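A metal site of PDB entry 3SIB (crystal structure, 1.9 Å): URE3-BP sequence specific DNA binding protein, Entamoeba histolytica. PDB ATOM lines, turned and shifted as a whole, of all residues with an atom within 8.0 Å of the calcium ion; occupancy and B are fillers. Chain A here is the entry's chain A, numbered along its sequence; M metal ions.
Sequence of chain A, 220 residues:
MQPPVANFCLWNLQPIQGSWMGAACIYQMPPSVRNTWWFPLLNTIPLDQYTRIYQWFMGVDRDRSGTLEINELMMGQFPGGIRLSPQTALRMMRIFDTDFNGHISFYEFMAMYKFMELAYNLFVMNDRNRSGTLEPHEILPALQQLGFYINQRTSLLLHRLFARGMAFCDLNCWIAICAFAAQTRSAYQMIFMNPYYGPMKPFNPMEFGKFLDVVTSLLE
Six residues have an atom within 4 Å of the calcium ion: Asp 61, Asp 63, Ser 65, Thr 67, Glu 69 and Glu 72.
The nearest printed residue that does not touch the calcium ion is Leu 68 (4.3 Å).
The calcium ion is bound by the side-chain carboxylate (OD1) of Asp 61, the side-chain carboxylate (OD1) of Asp 63, the side-chain carboxylate (OE1) of Glu 69, the backbone carbonyl oxygen (O) of Thr 67, the side-chain carboxylate (OE2) of Glu 72, the side-chain carboxylate (OE1) of Glu 72 and the side-chain hydroxyl (OG) of Ser 65.
The backbone NH (N) of Arg 64 lies close to the side-chain carboxylate (OD1) of Asp 61.
The backbone NH of Gly 66 is in hydrogen-bond range of the side-chain carboxylate of Asp 61.
OE2 of Glu 69 lies within hydrogen-bond range of ND1 of His 103.
The side-chain carboxylate (OE2) of Glu 72 lies close to the backbone NH (N) of Arg 62.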
ATOM      1  N   PHE A  57      15.268 -23.974  18.249  1.00  0.00           N
ATOM      2  CA  PHE A  57      16.208 -23.564  19.287  1.00  0.00           C
ATOM      3  C   PHE A  57      16.405 -22.052  19.263  1.00  0.00           C
ATOM      4  O   PHE A  57      16.340 -21.387  20.285  1.00  0.00           O
ATOM      5  CB  PHE A  57      17.539 -24.274  19.069  1.00  0.00           C
ATOM      6  CG  PHE A  57      18.634 -23.938  20.071  1.00  0.00           C
ATOM      7  CD1 PHE A  57      18.752 -24.655  21.244  1.00  0.00           C
ATOM      8  CD2 PHE A  57      19.583 -22.978  19.788  1.00  0.00           C
ATOM      9  CE1 PHE A  57      19.755 -24.411  22.146  1.00  0.00           C
ATOM     10  CE2 PHE A  57      20.644 -22.717  20.715  1.00  0.00           C
ATOM     11  CZ  PHE A  57      20.720 -23.450  21.882  1.00  0.00           C
ATOM     12  N   MET A  58      16.674 -21.507  18.084  1.00  0.00           N
ATOM     13  CA  MET A  58      16.896 -20.069  17.967  1.00  0.00           C
ATOM     14  C   MET A  58      15.676 -19.278  18.441  1.00  0.00           C
ATOM     15  O   MET A  58      15.840 -18.265  19.126  1.00  0.00           O
ATOM     16  CB  MET A  58      17.257 -19.695  16.533  1.00  0.00           C
ATOM     17  CG  MET A  58      18.662 -20.145  16.132  1.00  0.00           C
ATOM     18  SD  MET A  58      19.172 -19.436  14.541  1.00  0.00           S
ATOM     19  CE  MET A  58      17.748 -19.715  13.499  1.00  0.00           C
ATOM     20  N   VAL A  60      13.405 -20.131  20.780  1.00  0.00           N
ATOM     21  CA  VAL A  60      13.410 -20.190  22.237  1.00  0.00           C
ATOM     22  C   VAL A  60      14.527 -19.343  22.911  1.00  0.00           C
ATOM     23  O   VAL A  60      14.335 -18.793  24.000  1.00  0.00           O
ATOM     24  CB  VAL A  60      13.516 -21.691  22.712  1.00  0.00           C
ATOM     25  CG1 VAL A  60      13.435 -21.814  24.253  1.00  0.00           C
ATOM     26  CG2 VAL A  60      12.387 -22.530  22.068  1.00  0.00           C
ATOM     27  N   ASP A  61      15.687 -19.285  22.259  1.00  0.00           N
ATOM     28  CA  ASP A  61      16.864 -18.532  22.750  1.00  0.00           C
ATOM     29  C   ASP A  61      16.670 -17.020  22.556  1.00  0.00           C
ATOM     30  O   ASP A  61      17.312 -16.364  21.693  1.00  0.00           O
ATOM     31  CB  ASP A  61      18.096 -19.042  22.010  1.00  0.00           C
ATOM     32  CG  ASP A  61      19.387 -18.444  22.513  1.00  0.00           C
ATOM     33  OD1 ASP A  61      19.397 -17.844  23.635  1.00  0.00           O
ATOM     34  OD2 ASP A  61      20.406 -18.601  21.800  1.00  0.00           O
ATOM     35  N   ARG A  62      15.778 -16.444  23.362  1.00  0.00           N
ATOM     36  CA  ARG A  62      15.389 -15.060  23.175  1.00  0.00           C
ATOM     37  C   ARG A  62      16.564 -14.065  23.260  1.00  0.00           C
ATOM     38  O   ARG A  62      16.553 -13.034  22.572  1.00  0.00           O
ATOM     39  CB  ARG A  62      14.272 -14.691  24.149  1.00  0.00           C
ATOM     40  CG  ARG A  62      12.919 -15.345  23.747  1.00  0.00           C
ATOM     41  CD  ARG A  62      11.915 -15.303  24.861  1.00  0.00           C
ATOM     42  NE  ARG A  62      10.653 -15.947  24.435  1.00  0.00           N
ATOM     43  CZ  ARG A  62       9.617 -15.303  23.895  1.00  0.00           C
ATOM     44  NH1 ARG A  62       9.647 -13.978  23.732  1.00  0.00           N
ATOM     45  NH2 ARG A  62       8.527 -15.978  23.541  1.00  0.00           N
ATOM     46  N   ASP A  63      17.592 -14.353  24.051  1.00  0.00           N
ATOM     47  CA  ASP A  63      18.742 -13.433  24.161  1.00  0.00           C
ATOM     48  C   ASP A  63      19.919 -13.784  23.225  1.00  0.00           C
ATOM     49  O   ASP A  63      20.993 -13.194  23.328  1.00  0.00           O
ATOM     50  CB  ASP A  63      19.205 -13.284  25.617  1.00  0.00           C
ATOM     51  CG  ASP A  63      19.790 -14.557  26.194  1.00  0.00           C
ATOM     52  OD1 ASP A  63      19.995 -15.544  25.443  1.00  0.00           O
ATOM     53  OD2 ASP A  63      20.067 -14.555  27.404  1.00  0.00           O
ATOM     54  N   ARG A  64      19.707 -14.759  22.352  1.00  0.00           N
ATOM     55  CA  ARG A  64      20.674 -15.152  21.319  1.00  0.00           C
ATOM     56  C   ARG A  64      22.019 -15.583  21.913  1.00  0.00           C
ATOM     57  O   ARG A  64      23.052 -15.427  21.276  1.00  0.00           O
ATOM     58  CB  ARG A  64      20.856 -14.018  20.301  1.00  0.00           C
ATOM     59  CG  ARG A  64      19.534 -13.421  19.770  1.00  0.00           C
ATOM     60  CD  ARG A  64      19.807 -12.155  18.929  1.00  0.00           C
ATOM     61  NE  ARG A  64      20.896 -12.423  18.010  1.00  0.00           N
ATOM     62  CZ  ARG A  64      22.150 -11.951  18.083  1.00  0.00           C
ATOM     63  NH1 ARG A  64      22.514 -11.058  18.993  1.00  0.00           N
ATOM     64  NH2 ARG A  64      23.034 -12.337  17.172  1.00  0.00           N
ATOM     65  N   SER A  65      21.995 -16.109  23.141  1.00  0.00           N
ATOM     66  CA  SER A  65      23.232 -16.505  23.838  1.00  0.00           C
ATOM     67  C   SER A  65      23.849 -17.768  23.287  1.00  0.00           C
ATOM     68  O   SER A  65      24.995 -18.093  23.613  1.00  0.00           O
ATOM     69  CB  SER A  65      22.938 -16.714  25.343  1.00  0.00           C
ATOM     70  OG  SER A  65      22.154 -17.866  25.610  1.00  0.00           O
ATOM     71  N   GLY A  66      23.090 -18.501  22.470  1.00  0.00           N
ATOM     72  CA  GLY A  66      23.535 -19.812  21.966  1.00  0.00           C
ATOM     73  C   GLY A  66      23.272 -20.936  22.953  1.00  0.00           C
ATOM     74  O   GLY A  66      23.765 -22.068  22.774  1.00  0.00           O
ATOM     75  N   THR A  67      22.486 -20.635  23.990  1.00  0.00           N
ATOM     76  CA  THR A  67      22.118 -21.565  25.033  1.00  0.00           C
ATOM     77  C   THR A  67      20.692 -21.237  25.539  1.00  0.00           C
ATOM     78  O   THR A  67      20.239 -20.083  25.458  1.00  0.00           O
ATOM     79  CB  THR A  67      23.083 -21.462  26.239  1.00  0.00           C
ATOM     80  OG1 THR A  67      23.022 -20.130  26.782  1.00  0.00           O
ATOM     81  CG2 THR A  67      24.570 -21.802  25.838  1.00  0.00           C
ATOM     82  N   LEU A  68      19.969 -22.232  26.058  1.00  0.00           N
ATOM     83  CA  LEU A  68      18.648 -21.980  26.644  1.00  0.00           C
ATOM     84  C   LEU A  68      18.727 -21.956  28.147  1.00  0.00           C
ATOM     85  O   LEU A  68      19.312 -22.855  28.784  1.00  0.00           O
ATOM     86  CB  LEU A  68      17.566 -22.996  26.206  1.00  0.00           C
ATOM     87  CG  LEU A  68      17.526 -23.296  24.701  1.00  0.00           C
ATOM     88  CD1 LEU A  68      16.373 -24.260  24.423  1.00  0.00           C
ATOM     89  CD2 LEU A  68      17.398 -22.006  23.900  1.00  0.00           C
ATOM     90  N   GLU A  69      18.151 -20.899  28.720  1.00  0.00           N
ATOM     91  CA  GLU A  69      18.108 -20.724  30.169  1.00  0.00           C
ATOM     92  C   GLU A  69      16.698 -21.068  30.661  1.00  0.00           C
ATOM     93  O   GLU A  69      15.746 -21.163  29.877  1.00  0.00           O
ATOM     94  CB  GLU A  69      18.519 -19.279  30.550  1.00  0.00           C
ATOM     95  CG  GLU A  69      20.014 -19.017  30.423  1.00  0.00           C
ATOM     96  CD  GLU A  69      20.466 -19.022  28.970  1.00  0.00           C
ATOM     97  OE1 GLU A  69      19.987 -18.173  28.160  1.00  0.00           O
ATOM     98  OE2 GLU A  69      21.301 -19.892  28.641  1.00  0.00           O
ATOM     99  N   ILE A  70      16.525 -21.275  31.958  1.00  0.00           N
ATOM    100  CA  ILE A  70      15.226 -21.712  32.437  1.00  0.00           C
ATOM    101  C   ILE A  70      14.085 -20.732  32.107  1.00  0.00           C
ATOM    102  O   ILE A  70      13.017 -21.188  31.706  1.00  0.00           O
ATOM    103  CB  ILE A  70      15.262 -22.109  33.926  1.00  0.00           C
ATOM    104  CG1 ILE A  70      14.028 -22.980  34.245  1.00  0.00           C
ATOM    105  CG2 ILE A  70      15.417 -20.882  34.814  1.00  0.00           C
ATOM    106  CD1 ILE A  70      14.016 -23.625  35.616  1.00  0.00           C
ATOM    107  N   ASN A  71      14.323 -19.413  32.204  1.00  0.00           N
ATOM    108  CA  ASN A  71      13.325 -18.380  31.824  1.00  0.00           C
ATOM    109  C   ASN A  71      12.859 -18.524  30.375  1.00  0.00           C
ATOM    110  O   ASN A  71      11.680 -18.333  30.063  1.00  0.00           O
ATOM    111  CB  ASN A  71      13.803 -16.920  32.099  1.00  0.00           C
ATOM    112  CG  ASN A  71      14.891 -16.417  31.105  1.00  0.00           C
ATOM    113  OD1 ASN A  71      14.665 -15.483  30.280  1.00  0.00           O
ATOM    114  ND2 ASN A  71      16.063 -17.003  31.193  1.00  0.00           N
ATOM    115  N   GLU A  72      13.801 -18.857  29.501  1.00  0.00           N
ATOM    116  CA  GLU A  72      13.529 -19.074  28.074  1.00  0.00           C
ATOM    117  C   GLU A  72      12.699 -20.367  27.877  1.00  0.00           C
ATOM    118  O   GLU A  72      11.746 -20.399  27.081  1.00  0.00           O
ATOM    119  CB  GLU A  72      14.832 -19.119  27.282  1.00  0.00           C
ATOM    120  CG  GLU A  72      15.559 -17.745  27.203  1.00  0.00           C
ATOM    121  CD  GLU A  72      16.936 -17.833  26.588  1.00  0.00           C
ATOM    122  OE1 GLU A  72      17.470 -18.947  26.479  1.00  0.00           O
ATOM    123  OE2 GLU A  72      17.470 -16.761  26.197  1.00  0.00           O
ATOM    124  N   HIS A 103      22.457 -24.402  31.812  1.00  0.00           N
ATOM    125  CA  HIS A 103      22.153 -23.956  30.467  1.00  0.00           C
ATOM    126  C   HIS A 103      21.883 -25.194  29.608  1.00  0.00           C
ATOM    127  O   HIS A 103      22.497 -26.256  29.805  1.00  0.00           O
ATOM    128  CB  HIS A 103      23.298 -23.143  29.844  1.00  0.00           C
ATOM    129  CG  HIS A 103      23.716 -21.935  30.615  1.00  0.00           C
ATOM    130  ND1 HIS A 103      23.124 -20.695  30.459  1.00  0.00           N
ATOM    131  CD2 HIS A 103      24.670 -21.778  31.567  1.00  0.00           C
ATOM    132  CE1 HIS A 103      23.708 -19.829  31.268  1.00  0.00           C
ATOM    133  NE2 HIS A 103      24.665 -20.453  31.936  1.00  0.00           N
ATOM    134  N   ILE A 104      20.933 -25.088  28.686  1.00  0.00           N
ATOM    135  CA  ILE A 104      20.659 -26.159  27.715  1.00  0.00           C
ATOM    136  C   ILE A 104      21.381 -25.817  26.436  1.00  0.00           C
ATOM    137  O   ILE A 104      21.053 -24.833  25.799  1.00  0.00           O
ATOM    138  CB  ILE A 104      19.141 -26.322  27.466  1.00  0.00           C
ATOM    139  CG1 ILE A 104      18.454 -26.825  28.728  1.00  0.00           C
ATOM    140  CG2 ILE A 104      18.801 -27.277  26.275  1.00  0.00           C
ATOM    141  CD1 ILE A 104      18.820 -28.194  29.098  1.00  0.00           C
HETATM  142 CA    CA M   1      19.638 -17.832  25.859  1.00  0.00          CA
